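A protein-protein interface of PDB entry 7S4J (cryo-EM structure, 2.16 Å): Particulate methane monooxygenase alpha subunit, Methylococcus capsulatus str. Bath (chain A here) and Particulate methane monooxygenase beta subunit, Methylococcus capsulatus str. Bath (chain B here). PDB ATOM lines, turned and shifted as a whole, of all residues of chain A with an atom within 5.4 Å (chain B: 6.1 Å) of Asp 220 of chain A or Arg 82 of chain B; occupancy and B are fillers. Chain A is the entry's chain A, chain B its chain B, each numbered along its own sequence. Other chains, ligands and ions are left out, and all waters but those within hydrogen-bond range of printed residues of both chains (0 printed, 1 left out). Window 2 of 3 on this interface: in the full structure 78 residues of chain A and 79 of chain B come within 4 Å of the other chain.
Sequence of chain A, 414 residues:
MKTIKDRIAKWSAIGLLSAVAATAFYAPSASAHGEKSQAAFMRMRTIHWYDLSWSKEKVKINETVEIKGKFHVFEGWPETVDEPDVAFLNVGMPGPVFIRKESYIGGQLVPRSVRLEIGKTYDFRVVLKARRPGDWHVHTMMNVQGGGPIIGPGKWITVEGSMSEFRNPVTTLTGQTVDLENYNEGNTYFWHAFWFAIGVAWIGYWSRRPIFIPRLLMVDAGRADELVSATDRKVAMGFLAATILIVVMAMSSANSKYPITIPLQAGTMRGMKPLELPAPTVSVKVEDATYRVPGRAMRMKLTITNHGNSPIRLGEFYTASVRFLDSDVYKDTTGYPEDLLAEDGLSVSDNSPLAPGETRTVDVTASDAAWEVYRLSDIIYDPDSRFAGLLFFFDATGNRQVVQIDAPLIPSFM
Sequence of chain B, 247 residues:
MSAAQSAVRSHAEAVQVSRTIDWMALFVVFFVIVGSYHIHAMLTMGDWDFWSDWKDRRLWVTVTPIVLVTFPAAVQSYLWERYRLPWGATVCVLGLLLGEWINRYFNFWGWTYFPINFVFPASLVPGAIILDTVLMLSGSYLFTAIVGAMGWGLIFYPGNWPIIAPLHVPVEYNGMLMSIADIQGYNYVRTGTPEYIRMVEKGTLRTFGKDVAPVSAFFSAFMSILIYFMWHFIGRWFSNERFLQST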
ATOM      1  N   ARG A 215      13.605 -15.987   7.218  1.00  0.00           N
ATOM      2  CA  ARG A 215      14.558 -17.043   6.893  1.00  0.00           C
ATOM      3  C   ARG A 215      14.635 -18.078   8.006  1.00  0.00           C
ATOM      4  O   ARG A 215      14.730 -19.281   7.737  1.00  0.00           O
ATOM      5  CB  ARG A 215      15.933 -16.442   6.609  1.00  0.00           C
ATOM      6  CG  ARG A 215      16.012 -15.738   5.270  1.00  0.00           C
ATOM      7  CD  ARG A 215      17.391 -15.171   5.002  1.00  0.00           C
ATOM      8  NE  ARG A 215      18.300 -16.168   4.457  1.00  0.00           N
ATOM      9  CZ  ARG A 215      18.465 -16.395   3.163  1.00  0.00           C
ATOM     10  NH1 ARG A 215      17.770 -15.737   2.253  1.00  0.00           N
ATOM     11  NH2 ARG A 215      19.345 -17.310   2.772  1.00  0.00           N
ATOM     12  N   LEU A 216      14.589 -17.630   9.261  1.00  0.00           N
ATOM     13  CA  LEU A 216      14.556 -18.557  10.384  1.00  0.00           C
ATOM     14  C   LEU A 216      13.320 -19.441  10.325  1.00  0.00           C
ATOM     15  O   LEU A 216      13.407 -20.658  10.525  1.00  0.00           O
ATOM     16  CB  LEU A 216      14.589 -17.774  11.696  1.00  0.00           C
ATOM     17  CG  LEU A 216      14.395 -18.535  13.005  1.00  0.00           C
ATOM     18  CD1 LEU A 216      15.610 -19.376  13.326  1.00  0.00           C
ATOM     19  CD2 LEU A 216      14.096 -17.568  14.131  1.00  0.00           C
ATOM     20  N   LEU A 217      12.163 -18.846  10.033  1.00  0.00           N
ATOM     21  CA  LEU A 217      10.933 -19.625   9.958  1.00  0.00           C
ATOM     22  C   LEU A 217      10.956 -20.589   8.780  1.00  0.00           C
ATOM     23  O   LEU A 217      10.427 -21.698   8.875  1.00  0.00           O
ATOM     24  CB  LEU A 217       9.724 -18.697   9.868  1.00  0.00           C
ATOM     25  CG  LEU A 217       9.463 -17.832  11.102  1.00  0.00           C
ATOM     26  CD1 LEU A 217       8.344 -16.843  10.837  1.00  0.00           C
ATOM     27  CD2 LEU A 217       9.169 -18.680  12.324  1.00  0.00           C
ATOM     28  N   MET A 218      11.549 -20.185   7.657  1.00  0.00           N
ATOM     29  CA  MET A 218      11.636 -21.087   6.513  1.00  0.00           C
ATOM     30  C   MET A 218      12.580 -22.250   6.788  1.00  0.00           C
ATOM     31  O   MET A 218      12.298 -23.387   6.394  1.00  0.00           O
ATOM     32  CB  MET A 218      12.074 -20.323   5.267  1.00  0.00           C
ATOM     33  CG  MET A 218      11.028 -19.368   4.734  1.00  0.00           C
ATOM     34  SD  MET A 218      10.036 -20.085   3.413  1.00  0.00           S
ATOM     35  CE  MET A 218      11.312 -20.612   2.273  1.00  0.00           C
ATOM     36  N   VAL A 219      13.706 -21.992   7.456  1.00  0.00           N
ATOM     37  CA  VAL A 219      14.632 -23.075   7.774  1.00  0.00           C
ATOM     38  C   VAL A 219      14.013 -24.017   8.799  1.00  0.00           C
ATOM     39  O   VAL A 219      14.193 -25.238   8.726  1.00  0.00           O
ATOM     40  CB  VAL A 219      15.982 -22.511   8.256  1.00  0.00           C
ATOM     41  CG1 VAL A 219      16.873 -23.622   8.764  1.00  0.00           C
ATOM     42  CG2 VAL A 219      16.672 -21.766   7.141  1.00  0.00           C
ATOM     43  N   ASP A 220      13.267 -23.472   9.761  1.00  0.00           N
ATOM     44  CA  ASP A 220      12.611 -24.306  10.767  1.00  0.00           C
ATOM     45  C   ASP A 220      11.492 -25.139  10.147  1.00  0.00           C
ATOM     46  O   ASP A 220      11.486 -26.368  10.249  1.00  0.00           O
ATOM     47  CB  ASP A 220      12.069 -23.427  11.899  1.00  0.00           C
ATOM     48  CG  ASP A 220      13.162 -22.896  12.798  1.00  0.00           C
ATOM     49  OD1 ASP A 220      14.341 -23.240  12.572  1.00  0.00           O
ATOM     50  OD2 ASP A 220      12.844 -22.128  13.729  1.00  0.00           O
ATOM     51  N   ALA A 221      10.536 -24.475   9.502  1.00  0.00           N
ATOM     52  CA  ALA A 221       9.369 -25.138   8.940  1.00  0.00           C
ATOM     53  C   ALA A 221       9.746 -25.910   7.689  1.00  0.00           C
ATOM     54  O   ALA A 221       9.703 -25.369   6.579  1.00  0.00           O
ATOM     55  CB  ALA A 221       8.274 -24.121   8.619  1.00  0.00           C
ATOM     56  N   GLY A 222      10.105 -27.173   7.857  1.00  0.00           N
ATOM     57  CA  GLY A 222      10.507 -27.990   6.738  1.00  0.00           C
ATOM     58  C   GLY A 222      11.869 -27.584   6.221  1.00  0.00           C
ATOM     59  O   GLY A 222      12.576 -26.757   6.794  1.00  0.00           O
ATOM     60  N   SER B  77      28.649 -21.160  11.932  1.00  0.00           N
ATOM     61  CA  SER B  77      27.899 -22.317  12.401  1.00  0.00           C
ATOM     62  C   SER B  77      26.516 -21.925  12.886  1.00  0.00           C
ATOM     63  O   SER B  77      25.584 -22.733  12.827  1.00  0.00           O
ATOM     64  CB  SER B  77      28.668 -23.026  13.512  1.00  0.00           C
ATOM     65  OG  SER B  77      28.327 -22.510  14.782  1.00  0.00           O
ATOM     66  N   TYR B  78      26.361 -20.698  13.375  1.00  0.00           N
ATOM     67  CA  TYR B  78      25.027 -20.254  13.771  1.00  0.00           C
ATOM     68  C   TYR B  78      24.228 -19.727  12.583  1.00  0.00           C
ATOM     69  O   TYR B  78      23.109 -20.184  12.320  1.00  0.00           O
ATOM     70  CB  TYR B  78      25.129 -19.191  14.862  1.00  0.00           C
ATOM     71  CG  TYR B  78      23.848 -18.435  15.106  1.00  0.00           C
ATOM     72  CD1 TYR B  78      22.781 -19.037  15.753  1.00  0.00           C
ATOM     73  CD2 TYR B  78      23.709 -17.114  14.708  1.00  0.00           C
ATOM     74  CE1 TYR B  78      21.611 -18.352  15.987  1.00  0.00           C
ATOM     75  CE2 TYR B  78      22.542 -16.420  14.939  1.00  0.00           C
ATOM     76  CZ  TYR B  78      21.497 -17.046  15.579  1.00  0.00           C
ATOM     77  OH  TYR B  78      20.329 -16.364  15.814  1.00  0.00           O
ATOM     78  N   LEU B  79      24.784 -18.753  11.862  1.00  0.00           N
ATOM     79  CA  LEU B  79      24.020 -18.029  10.853  1.00  0.00           C
ATOM     80  C   LEU B  79      23.632 -18.929   9.693  1.00  0.00           C
ATOM     81  O   LEU B  79      22.470 -18.951   9.280  1.00  0.00           O
ATOM     82  CB  LEU B  79      24.815 -16.826  10.347  1.00  0.00           C
ATOM     83  CG  LEU B  79      24.813 -15.571  11.215  1.00  0.00           C
ATOM     84  CD1 LEU B  79      25.553 -14.450  10.512  1.00  0.00           C
ATOM     85  CD2 LEU B  79      23.398 -15.151  11.563  1.00  0.00           C
ATOM     86  N   TRP B  80      24.589 -19.679   9.142  1.00  0.00           N
ATOM     87  CA  TRP B  80      24.260 -20.544   8.016  1.00  0.00           C
ATOM     88  C   TRP B  80      23.230 -21.590   8.421  1.00  0.00           C
ATOM     89  O   TRP B  80      22.228 -21.788   7.728  1.00  0.00           O
ATOM     90  CB  TRP B  80      25.518 -21.209   7.467  1.00  0.00           C
ATOM     91  CG  TRP B  80      25.232 -22.119   6.322  1.00  0.00           C
ATOM     92  CD1 TRP B  80      25.321 -23.474   6.313  1.00  0.00           C
ATOM     93  CD2 TRP B  80      24.789 -21.735   5.016  1.00  0.00           C
ATOM     94  NE1 TRP B  80      24.969 -23.963   5.082  1.00  0.00           N
ATOM     95  CE2 TRP B  80      24.637 -22.914   4.267  1.00  0.00           C
ATOM     96  CE3 TRP B  80      24.507 -20.509   4.408  1.00  0.00           C
ATOM     97  CZ2 TRP B  80      24.219 -22.905   2.941  1.00  0.00           C
ATOM     98  CZ3 TRP B  80      24.093 -20.502   3.095  1.00  0.00           C
ATOM     99  CH2 TRP B  80      23.953 -21.693   2.374  1.00  0.00           C
ATOM    100  N   GLU B  81      23.432 -22.227   9.576  1.00  0.00           N
ATOM    101  CA  GLU B  81      22.531 -23.293   9.998  1.00  0.00           C
ATOM    102  C   GLU B  81      21.120 -22.786  10.262  1.00  0.00           C
ATOM    103  O   GLU B  81      20.150 -23.463   9.909  1.00  0.00           O
ATOM    104  CB  GLU B  81      23.075 -23.983  11.246  1.00  0.00           C
ATOM    105  CG  GLU B  81      22.603 -25.420  11.433  1.00  0.00           C
ATOM    106  CD  GLU B  81      23.207 -26.394  10.427  1.00  0.00           C
ATOM    107  OE1 GLU B  81      23.035 -26.204   9.205  1.00  0.00           O
ATOM    108  OE2 GLU B  81      23.869 -27.357  10.866  1.00  0.00           O
ATOM    109  N   ARG B  82      20.975 -21.612  10.876  1.00  0.00           N
ATOM    110  CA  ARG B  82      19.654 -21.170  11.298  1.00  0.00           C
ATOM    111  C   ARG B  82      18.943 -20.277  10.290  1.00  0.00           C
ATOM    112  O   ARG B  82      17.713 -20.193  10.335  1.00  0.00           O
ATOM    113  CB  ARG B  82      19.741 -20.438  12.641  1.00  0.00           C
ATOM    114  CG  ARG B  82      20.181 -21.310  13.806  1.00  0.00           C
ATOM    115  CD  ARG B  82      19.477 -22.657  13.805  1.00  0.00           C
ATOM    116  NE  ARG B  82      18.037 -22.536  13.995  1.00  0.00           N
ATOM    117  CZ  ARG B  82      17.434 -22.513  15.176  1.00  0.00           C
ATOM    118  NH1 ARG B  82      18.118 -22.604  16.303  1.00  0.00           N
ATOM    119  NH2 ARG B  82      16.111 -22.397  15.226  1.00  0.00           N
ATOM    120  N   TYR B  83      19.661 -19.616   9.381  1.00  0.00           N
ATOM    121  CA  TYR B  83      19.020 -18.702   8.448  1.00  0.00           C
ATOM    122  C   TYR B  83      19.501 -18.849   7.013  1.00  0.00           C
ATOM    123  O   TYR B  83      18.978 -18.146   6.144  1.00  0.00           O
ATOM    124  CB  TYR B  83      19.239 -17.244   8.884  1.00  0.00           C
ATOM    125  CG  TYR B  83      19.044 -16.973  10.355  1.00  0.00           C
ATOM    126  CD1 TYR B  83      20.073 -17.174  11.261  1.00  0.00           C
ATOM    127  CD2 TYR B  83      17.839 -16.491  10.834  1.00  0.00           C
ATOM    128  CE1 TYR B  83      19.898 -16.926  12.598  1.00  0.00           C
ATOM    129  CE2 TYR B  83      17.659 -16.234  12.171  1.00  0.00           C
ATOM    130  CZ  TYR B  83      18.691 -16.454  13.049  1.00  0.00           C
ATOM    131  OH  TYR B  83      18.515 -16.201  14.385  1.00  0.00           O
ATOM    132  N   ARG B  84      20.467 -19.725   6.735  1.00  0.00           N
ATOM    133  CA  ARG B  84      21.114 -19.802   5.428  1.00  0.00           C
ATOM    134  C   ARG B  84      21.644 -18.436   4.998  1.00  0.00           C
ATOM    135  O   ARG B  84      21.517 -18.029   3.842  1.00  0.00           O
ATOM    136  CB  ARG B  84      20.173 -20.389   4.376  1.00  0.00           C
ATOM    137  CG  ARG B  84      19.806 -21.838   4.623  1.00  0.00           C
ATOM    138  CD  ARG B  84      20.938 -22.768   4.225  1.00  0.00           C
ATOM    139  NE  ARG B  84      20.692 -24.146   4.634  1.00  0.00           N
ATOM    140  CZ  ARG B  84      20.769 -24.589   5.880  1.00  0.00           C
ATOM    141  NH1 ARG B  84      21.116 -23.795   6.878  1.00  0.00           N
ATOM    142  NH2 ARG B  84      20.488 -25.864   6.133  1.00  0.00           N
ATOM    143  N   LEU B  85      22.244 -17.720   5.945  1.00  0.00           N
ATOM    144  CA  LEU B  85      22.891 -16.441   5.670  1.00  0.00           C
ATOM    145  C   LEU B  85      24.391 -16.674   5.601  1.00  0.00           C
ATOM    146  O   LEU B  85      25.018 -16.975   6.627  1.00  0.00           O
ATOM    147  CB  LEU B  85      22.555 -15.412   6.752  1.00  0.00           C
ATOM    148  CG  LEU B  85      21.129 -14.867   6.731  1.00  0.00           C
ATOM    149  CD1 LEU B  85      20.849 -14.098   8.001  1.00  0.00           C
ATOM    150  CD2 LEU B  85      20.915 -13.997   5.512  1.00  0.00           C
ATOM    151  N   TYR B 141      29.925 -28.314   6.364  1.00  0.00           N
ATOM    152  CA  TYR B 141      30.787 -27.679   7.352  1.00  0.00           C
ATOM    153  C   TYR B 141      32.158 -28.338   7.408  1.00  0.00           C
ATOM    154  O   TYR B 141      33.154 -27.655   7.653  1.00  0.00           O
ATOM    155  CB  TYR B 141      30.134 -27.716   8.731  1.00  0.00           C
ATOM    156  CG  TYR B 141      29.124 -26.621   8.952  1.00  0.00           C
ATOM    157  CD1 TYR B 141      29.524 -25.304   9.102  1.00  0.00           C
ATOM    158  CD2 TYR B 141      27.769 -26.906   9.013  1.00  0.00           C
ATOM    159  CE1 TYR B 141      28.602 -24.302   9.303  1.00  0.00           C
ATOM    160  CE2 TYR B 141      26.842 -25.913   9.213  1.00  0.00           C
ATOM    161  CZ  TYR B 141      27.263 -24.612   9.358  1.00  0.00           C
ATOM    162  OH  TYR B 141      26.341 -23.618   9.559  1.00  0.00           O
ATOM    163  N   SER B 239      24.841 -21.274  20.511  1.00  0.00           N
ATOM    164  CA  SER B 239      23.556 -21.061  19.862  1.00  0.00           C
ATOM    165  C   SER B 239      22.399 -21.764  20.563  1.00  0.00           C
ATOM    166  O   SER B 239      21.279 -21.736  20.048  1.00  0.00           O
ATOM    167  CB  SER B 239      23.619 -21.521  18.405  1.00  0.00           C
ATOM    168  OG  SER B 239      24.744 -20.974  17.746  1.00  0.00           O
ATOM    169  N   GLU B 241      19.309 -22.623  23.120  1.00  0.00           N
ATOM    170  CA  GLU B 241      18.165 -21.821  23.544  1.00  0.00           C
ATOM    171  C   GLU B 241      17.507 -22.417  24.778  1.00  0.00           C
ATOM    172  O   GLU B 241      16.293 -22.319  24.965  1.00  0.00           O
ATOM    173  CB  GLU B 241      17.142 -21.690  22.420  1.00  0.00           C
ATOM    174  CG  GLU B 241      17.661 -20.999  21.184  1.00  0.00           C
ATOM    175  CD  GLU B 241      17.424 -21.808  19.926  1.00  0.00           C
ATOM    176  OE1 GLU B 241      16.296 -22.305  19.741  1.00  0.00           O
ATOM    177  OE2 GLU B 241      18.366 -21.946  19.119  1.00  0.00           O
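Of the 8 printed residues of chain A, 4 touch a printed residue of chain B. Printed residues of chain A that touch a printed residue of chain B: Arg 215, Leu 216, Val 219 and Asp 220. Hydrophobic or aromatic side chains of chain A within 4 Å of the printed part of chain B: Leu 216 and Val 219. Among the printed residues, 8 pairs touch across the chains. Among the printed residues, Asp or Glu carboxylates within 4 Å of a Lys or Arg side-chain nitrogen of the other chain: Asp 220 of chain A with Arg 82 of chain B.
The guanidinium group of Arg 215 of chain A is in hydrogen-bond range of the backbone carbonyl oxygen of Arg 84 of chain B (2.5 Å). NE of Arg 215 of chain A is in hydrogen-bond range of O of Tyr 83 of chain B (2.7 Å). NH2 of Arg 82 of chain B lies within salt-bridge range of OD1 of Asp 220 of chain A (3.3 Å).
Among the printed residues, pairs that only touch across the chains: Arg 215 of chain A with Leu 85 of chain B (3.6 Å), Leu 216 of chain A with Arg 82 of chain B (3.6 Å), Leu 216 of chain A with Tyr 83 of chain B (3.5 Å), Val 219 of chain A with Glu 81 of chain B (3.5 Å) and Val 219 of chain A with Arg 82 of chain B (3.6 Å).
Of the printed residues of chain B, Val 219 of chain A touches Glu 81 (3.5 Å) and Arg 82 (3.6 Å). Asp 220 of chain A touches one residue of chain B. Ala 221 of chain A touches none of the printed residues of chain B. Printed residues of chain A within 4 Å of Glu 81 of chain B: Val 219 (3.5 Å). Glu 241 of chain B touches none of the printed residues of chain A. The nearest printed residue of chain B that does not touch Asp 220 of chain A is Glu 81 of chain B (6.4 Å). The nearest residue of chain A that does not touch Arg 82 of chain B is Arg 215 of chain A (4.1 Å). The nearest printed residue of chain B that does not touch Leu 216 of chain A is Tyr 78 of chain B (6.1 Å).
The guanidinium group (NH1) of Arg 82 of chain B lies within salt-bridge range of the side-chain carboxylate (OE2) of Glu 241 of chain B. The guanidinium group (NH1) of Arg 84 of chain B lies within salt-bridge range of the side-chain carboxylate (OE1) of Glu 81 of chain B. O of Leu 79 of chain B sits at hydrogen-bond distance from N of Arg 84 of chain B. The side-chain hydroxyl (OH) of Tyr 141 of chain B sits at hydrogen-bond distance from the backbone NH (N) of Glu 81 of chain B (3.2 Å). The guanidinium group (NH1) of Arg 84 of chain B sits at hydrogen-bond distance from the backbone carbonyl oxygen (O) of Trp 80 of chain B (2.4 Å).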
